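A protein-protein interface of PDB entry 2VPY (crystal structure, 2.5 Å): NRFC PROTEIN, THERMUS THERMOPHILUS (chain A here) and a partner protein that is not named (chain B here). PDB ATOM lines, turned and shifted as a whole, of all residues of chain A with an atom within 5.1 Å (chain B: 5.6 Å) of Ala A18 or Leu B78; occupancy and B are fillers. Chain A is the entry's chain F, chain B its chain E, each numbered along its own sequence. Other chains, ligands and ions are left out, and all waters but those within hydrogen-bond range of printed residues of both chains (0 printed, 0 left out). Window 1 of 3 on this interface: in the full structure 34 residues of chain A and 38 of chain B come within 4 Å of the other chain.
The backbone carbonyl oxygen (O) of Leu B78 lies within hydrogen-bond range of the side-chain hydroxyl (OG1) of Thr A134 (2.9 Å).
The side-chain amide oxygen (OE1) of Gln B83 sits at hydrogen-bond distance from the side-chain hydroxyl (OG1) of Thr A134, at 3.1 Å.
The backbone carbonyl oxygen of Ser B74 lies close to the side-chain amide oxygen of Gln B220 (3.1 Å).
The backbone carbonyl oxygen (O) of Arg B77 sits at hydrogen-bond distance from the side-chain amide nitrogen (ND2) of Asn B216 (3.2 Å).
The backbone NH of Gly B82 lies close to the side-chain sulfur of Cys B79, 3.7 Å away.
OD1 of Asn B216 sits close to OE1 of Gln B220, 3.0 Å away.
The backbone NH of Ala A18 lies close to the side-chain sulfur of Cys A16, 3.7 Å away.
Among the printed residues, pairs that only touch across the chains: Pro A136 with Gln B220 (3.2 Å), Pro A136 with Leu B78 (3.3 Å), Thr A134 with Arg B77 (3.4 Å), Val A21 with Pro B80 (3.4 Å), Ala A22 with Gln B83 (3.5 Å), Ala A18 with Pro B80 (3.5 Å), Ala A17 with Pro B80 (3.6 Å), Val A21 with Gln B83 (3.6 Å), Ala A18 with Leu B78 (3.7 Å) and Ala A18 with Cys B79 (3.8 Å).
Printed residues of chain B within 4 Å of Ala A18: Leu B78 (3.7 Å), Cys B79 (3.8 Å) and Pro B80 (3.5 Å).
Leu B78 touches three residues of chain A.
Of the printed residues of chain A, Cys B79 touches Ala A18.
Printed residues of chain B within 4 Å of Ala A17: Pro B80 (3.6 Å).
Gly B67 touches none of the printed residues of chain A.
The nearest residue of chain B that does not touch Ala A18 is Gln B83 (4.1 Å).
The nearest printed residue of chain A that does not touch Leu B78 is Cys A19 (6.2 Å).
Of the 10 printed residues of chain A, 6 touch a printed residue of chain B.
Hydrophobic or aromatic side chains of chain A within 4 Å of the printed part of chain B: Ala A18, Val A21, Ala A22 and Pro A136.
Among the printed residues, 12 pairs touch across the chains.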
ATOM      1  N   CYS A  16       2.850 -20.938  29.924  1.00  0.00           N
ATOM      2  CA  CYS A  16       3.440 -21.659  28.769  1.00  0.00           C
ATOM      3  C   CYS A  16       3.196 -23.047  29.398  1.00  0.00           C
ATOM      4  O   CYS A  16       3.255 -23.112  30.602  1.00  0.00           O
ATOM      5  CB  CYS A  16       4.950 -21.383  28.797  1.00  0.00           C
ATOM      6  SG  CYS A  16       5.712 -21.972  30.517  1.00  0.00           S
ATOM      7  N   ALA A  17       2.937 -24.181  28.789  1.00  0.00           N
ATOM      8  CA  ALA A  17       2.763 -25.217  29.836  1.00  0.00           C
ATOM      9  C   ALA A  17       3.947 -26.155  30.077  1.00  0.00           C
ATOM     10  O   ALA A  17       3.776 -27.372  30.113  1.00  0.00           O
ATOM     11  CB  ALA A  17       1.495 -26.023  29.601  1.00  0.00           C
ATOM     12  N   ALA A  18       5.123 -25.586  30.333  1.00  0.00           N
ATOM     13  CA  ALA A  18       6.340 -26.395  30.470  1.00  0.00           C
ATOM     14  C   ALA A  18       6.450 -27.398  31.598  1.00  0.00           C
ATOM     15  O   ALA A  18       6.982 -28.510  31.405  1.00  0.00           O
ATOM     16  CB  ALA A  18       7.558 -25.504  30.460  1.00  0.00           C
ATOM     17  N   CYS A  19       5.981 -26.960  32.761  1.00  0.00           N
ATOM     18  CA  CYS A  19       5.949 -27.723  33.995  1.00  0.00           C
ATOM     19  C   CYS A  19       4.984 -28.872  33.725  1.00  0.00           C
ATOM     20  O   CYS A  19       5.297 -30.044  33.944  1.00  0.00           O
ATOM     21  CB  CYS A  19       5.456 -26.827  35.146  1.00  0.00           C
ATOM     22  SG  CYS A  19       3.836 -25.978  34.886  1.00  0.00           S
ATOM     23  N   ALA A  20       3.813 -28.527  33.209  1.00  0.00           N
ATOM     24  CA  ALA A  20       2.799 -29.523  32.892  1.00  0.00           C
ATOM     25  C   ALA A  20       3.343 -30.596  31.956  1.00  0.00           C
ATOM     26  O   ALA A  20       3.082 -31.781  32.170  1.00  0.00           O
ATOM     27  CB  ALA A  20       1.570 -28.861  32.263  1.00  0.00           C
ATOM     28  N   VAL A  21       4.091 -30.209  30.920  1.00  0.00           N
ATOM     29  CA  VAL A  21       4.635 -31.204  29.996  1.00  0.00           C
ATOM     30  C   VAL A  21       5.824 -31.961  30.625  1.00  0.00           C
ATOM     31  O   VAL A  21       5.949 -33.162  30.439  1.00  0.00           O
ATOM     32  CB  VAL A  21       5.004 -30.558  28.588  1.00  0.00           C
ATOM     33  CG1 VAL A  21       5.544 -31.622  27.619  1.00  0.00           C
ATOM     34  CG2 VAL A  21       3.762 -29.906  27.964  1.00  0.00           C
ATOM     35  N   ALA A  22       6.668 -31.279  31.401  1.00  0.00           N
ATOM     36  CA  ALA A  22       7.806 -31.937  32.074  1.00  0.00           C
ATOM     37  C   ALA A  22       7.293 -33.080  33.011  1.00  0.00           C
ATOM     38  O   ALA A  22       7.883 -34.172  33.050  1.00  0.00           O
ATOM     39  CB  ALA A  22       8.652 -30.893  32.839  1.00  0.00           C
ATOM     40  N   CYS A  23       6.194 -32.805  33.734  1.00  0.00           N
ATOM     41  CA  CYS A  23       5.504 -33.767  34.619  1.00  0.00           C
ATOM     42  C   CYS A  23       5.088 -35.030  33.809  1.00  0.00           C
ATOM     43  O   CYS A  23       5.466 -36.148  34.149  1.00  0.00           O
ATOM     44  CB  CYS A  23       4.229 -33.142  35.224  1.00  0.00           C
ATOM     45  SG  CYS A  23       3.409 -34.172  36.512  1.00  0.00           S
ATOM     46  N   THR A 134      12.373 -27.567  35.181  1.00  0.00           N
ATOM     47  CA  THR A 134      12.188 -27.026  33.838  1.00  0.00           C
ATOM     48  C   THR A 134      11.749 -25.575  33.696  1.00  0.00           C
ATOM     49  O   THR A 134      11.939 -24.965  32.637  1.00  0.00           O
ATOM     50  CB  THR A 134      11.092 -27.784  33.069  1.00  0.00           C
ATOM     51  OG1 THR A 134      11.176 -27.466  31.677  1.00  0.00           O
ATOM     52  CG2 THR A 134       9.711 -27.325  33.552  1.00  0.00           C
ATOM     53  N   PRO A 136      11.108 -22.099  32.955  1.00  0.00           N
ATOM     54  CA  PRO A 136      11.801 -21.028  32.245  1.00  0.00           C
ATOM     55  C   PRO A 136      11.701 -19.704  32.970  1.00  0.00           C
ATOM     56  O   PRO A 136      12.667 -18.946  33.022  1.00  0.00           O
ATOM     57  CB  PRO A 136      11.083 -20.985  30.892  1.00  0.00           C
ATOM     58  CG  PRO A 136      10.598 -22.370  30.731  1.00  0.00           C
ATOM     59  CD  PRO A 136      10.029 -22.615  32.101  1.00  0.00           C
ATOM     60  N   CYS B  51      17.920 -25.330  21.512  1.00  0.00           N
ATOM     61  CA  CYS B  51      18.386 -25.315  22.907  1.00  0.00           C
ATOM     62  C   CYS B  51      19.264 -26.558  23.117  1.00  0.00           C
ATOM     63  O   CYS B  51      18.973 -27.599  22.533  1.00  0.00           O
ATOM     64  CB  CYS B  51      17.188 -25.381  23.865  1.00  0.00           C
ATOM     65  SG  CYS B  51      16.161 -23.887  23.906  1.00  0.00           S
ATOM     66  N   GLY B  52      20.317 -26.447  23.931  1.00  0.00           N
ATOM     67  CA  GLY B  52      21.184 -27.581  24.222  1.00  0.00           C
ATOM     68  C   GLY B  52      20.506 -28.421  25.290  1.00  0.00           C
ATOM     69  O   GLY B  52      20.054 -27.882  26.301  1.00  0.00           O
ATOM     70  N   ILE B  53      20.446 -29.731  25.108  1.00  0.00           N
ATOM     71  CA  ILE B  53      19.733 -30.573  26.061  1.00  0.00           C
ATOM     72  C   ILE B  53      20.476 -31.848  26.446  1.00  0.00           C
ATOM     73  O   ILE B  53      21.547 -32.128  25.919  1.00  0.00           O
ATOM     74  CB  ILE B  53      18.348 -30.998  25.419  1.00  0.00           C
ATOM     75  CG1 ILE B  53      18.590 -31.740  24.097  1.00  0.00           C
ATOM     76  CG2 ILE B  53      17.470 -29.756  25.139  1.00  0.00           C
ATOM     77  CD1 ILE B  53      17.371 -32.473  23.496  1.00  0.00           C
ATOM     78  N   VAL B  65      13.898 -35.391  28.471  1.00  0.00           N
ATOM     79  CA  VAL B  65      14.933 -34.559  27.896  1.00  0.00           C
ATOM     80  C   VAL B  65      15.074 -33.386  28.901  1.00  0.00           C
ATOM     81  O   VAL B  65      14.114 -33.024  29.567  1.00  0.00           O
ATOM     82  CB  VAL B  65      14.510 -34.202  26.433  1.00  0.00           C
ATOM     83  CG1 VAL B  65      14.131 -32.737  26.309  1.00  0.00           C
ATOM     84  CG2 VAL B  65      15.605 -34.668  25.464  1.00  0.00           C
ATOM     85  N   GLU B  66      16.264 -32.833  29.064  1.00  0.00           N
ATOM     86  CA  GLU B  66      16.444 -31.780  30.056  1.00  0.00           C
ATOM     87  C   GLU B  66      17.441 -30.723  29.603  1.00  0.00           C
ATOM     88  O   GLU B  66      18.356 -31.025  28.852  1.00  0.00           O
ATOM     89  CB  GLU B  66      16.937 -32.396  31.380  1.00  0.00           C
ATOM     90  CG  GLU B  66      16.523 -31.641  32.653  1.00  0.00           C
ATOM     91  CD  GLU B  66      15.060 -31.894  33.068  1.00  0.00           C
ATOM     92  OE1 GLU B  66      14.704 -33.061  33.345  1.00  0.00           O
ATOM     93  OE2 GLU B  66      14.273 -30.925  33.116  1.00  0.00           O
ATOM     94  N   GLY B  67      17.252 -29.485  30.039  1.00  0.00           N
ATOM     95  CA  GLY B  67      18.203 -28.452  29.692  1.00  0.00           C
ATOM     96  C   GLY B  67      19.436 -28.694  30.560  1.00  0.00           C
ATOM     97  O   GLY B  67      19.384 -29.542  31.451  1.00  0.00           O
ATOM     98  N   SER B  74      19.718 -23.228  27.044  1.00  0.00           N
ATOM     99  CA  SER B  74      18.764 -23.771  28.001  1.00  0.00           C
ATOM    100  C   SER B  74      19.045 -23.530  29.515  1.00  0.00           C
ATOM    101  O   SER B  74      18.093 -23.470  30.288  1.00  0.00           O
ATOM    102  CB  SER B  74      18.518 -25.272  27.739  1.00  0.00           C
ATOM    103  OG  SER B  74      19.651 -26.066  28.005  1.00  0.00           O
ATOM    104  N   GLY B  76      19.728 -25.167  32.171  1.00  0.00           N
ATOM    105  CA  GLY B  76      18.967 -26.008  33.084  1.00  0.00           C
ATOM    106  C   GLY B  76      17.462 -26.113  32.847  1.00  0.00           C
ATOM    107  O   GLY B  76      16.819 -27.073  33.279  1.00  0.00           O
ATOM    108  N   ARG B  77      16.905 -25.143  32.131  1.00  0.00           N
ATOM    109  CA  ARG B  77      15.466 -25.070  31.870  1.00  0.00           C
ATOM    110  C   ARG B  77      15.060 -25.476  30.437  1.00  0.00           C
ATOM    111  O   ARG B  77      15.910 -25.606  29.556  1.00  0.00           O
ATOM    112  CB  ARG B  77      15.003 -23.631  32.183  1.00  0.00           C
ATOM    113  CG  ARG B  77      15.651 -23.012  33.453  1.00  0.00           C
ATOM    114  CD  ARG B  77      15.178 -23.775  34.683  1.00  0.00           C
ATOM    115  NE  ARG B  77      15.642 -23.264  35.980  1.00  0.00           N
ATOM    116  CZ  ARG B  77      14.859 -22.923  37.011  1.00  0.00           C
ATOM    117  NH1 ARG B  77      13.529 -23.005  36.936  1.00  0.00           N
ATOM    118  NH2 ARG B  77      15.416 -22.540  38.156  1.00  0.00           N
ATOM    119  N   LEU B  78      13.768 -25.676  30.200  1.00  0.00           N
ATOM    120  CA  LEU B  78      13.304 -26.063  28.877  1.00  0.00           C
ATOM    121  C   LEU B  78      11.878 -25.580  28.665  1.00  0.00           C
ATOM    122  O   LEU B  78      11.155 -25.381  29.633  1.00  0.00           O
ATOM    123  CB  LEU B  78      13.342 -27.572  28.739  1.00  0.00           C
ATOM    124  CG  LEU B  78      13.946 -28.096  27.448  1.00  0.00           C
ATOM    125  CD1 LEU B  78      15.425 -27.705  27.264  1.00  0.00           C
ATOM    126  CD2 LEU B  78      13.785 -29.588  27.514  1.00  0.00           C
ATOM    127  N   CYS B  79      11.448 -25.382  27.421  1.00  0.00           N
ATOM    128  CA  CYS B  79      10.078 -24.937  27.249  1.00  0.00           C
ATOM    129  C   CYS B  79       9.170 -26.175  27.091  1.00  0.00           C
ATOM    130  O   CYS B  79       9.661 -27.305  27.064  1.00  0.00           O
ATOM    131  CB  CYS B  79       9.954 -23.954  26.065  1.00  0.00           C
ATOM    132  SG  CYS B  79       9.750 -24.675  24.354  1.00  0.00           S
ATOM    133  N   PRO B  80       7.831 -25.978  26.994  1.00  0.00           N
ATOM    134  CA  PRO B  80       6.908 -27.119  26.856  1.00  0.00           C
ATOM    135  C   PRO B  80       7.134 -28.021  25.635  1.00  0.00           C
ATOM    136  O   PRO B  80       7.069 -29.260  25.729  1.00  0.00           O
ATOM    137  CB  PRO B  80       5.513 -26.480  26.854  1.00  0.00           C
ATOM    138  CG  PRO B  80       5.708 -25.035  26.687  1.00  0.00           C
ATOM    139  CD  PRO B  80       7.129 -24.681  26.951  1.00  0.00           C
ATOM    140  N   GLY B  82       9.954 -28.380  23.945  1.00  0.00           N
ATOM    141  CA  GLY B  82      11.180 -29.130  24.059  1.00  0.00           C
ATOM    142  C   GLY B  82      10.946 -30.397  24.869  1.00  0.00           C
ATOM    143  O   GLY B  82      11.487 -31.473  24.546  1.00  0.00           O
ATOM    144  N   GLN B  83      10.119 -30.290  25.908  1.00  0.00           N
ATOM    145  CA  GLN B  83       9.841 -31.447  26.774  1.00  0.00           C
ATOM    146  C   GLN B  83       9.012 -32.507  26.055  1.00  0.00           C
ATOM    147  O   GLN B  83       9.183 -33.707  26.293  1.00  0.00           O
ATOM    148  CB  GLN B  83       9.108 -31.020  28.059  1.00  0.00           C
ATOM    149  CG  GLN B  83       9.897 -30.128  29.020  1.00  0.00           C
ATOM    150  CD  GLN B  83      10.815 -30.896  29.964  1.00  0.00           C
ATOM    151  OE1 GLN B  83      11.683 -30.311  30.624  1.00  0.00           O
ATOM    152  NE2 GLN B  83      10.617 -32.210  30.041  1.00  0.00           N
ATOM    153  N   ASN B 216      12.875 -20.461  24.512  1.00  0.00           N
ATOM    154  CA  ASN B 216      13.406 -20.670  25.850  1.00  0.00           C
ATOM    155  C   ASN B 216      14.249 -19.591  26.563  1.00  0.00           C
ATOM    156  O   ASN B 216      13.821 -19.049  27.586  1.00  0.00           O
ATOM    157  CB  ASN B 216      14.052 -22.070  25.829  1.00  0.00           C
ATOM    158  CG  ASN B 216      14.459 -22.588  27.190  1.00  0.00           C
ATOM    159  OD1 ASN B 216      13.965 -22.143  28.233  1.00  0.00           O
ATOM    160  ND2 ASN B 216      15.364 -23.574  27.183  1.00  0.00           N
ATOM    161  N   GLN B 220      13.181 -16.783  29.720  1.00  0.00           N
ATOM    162  CA  GLN B 220      13.977 -16.714  30.955  1.00  0.00           C
ATOM    163  C   GLN B 220      14.502 -15.287  31.162  1.00  0.00           C
ATOM    164  O   GLN B 220      14.530 -14.756  32.272  1.00  0.00           O
ATOM    165  CB  GLN B 220      15.198 -17.643  30.900  1.00  0.00           C
ATOM    166  CG  GLN B 220      14.885 -19.096  30.663  1.00  0.00           C
ATOM    167  CD  GLN B 220      16.121 -19.998  30.655  1.00  0.00           C
ATOM    168  OE1 GLN B 220      16.049 -21.152  30.213  1.00  0.00           O
ATOM    169  NE2 GLN B 220      17.250 -19.489  31.159  1.00  0.00           N
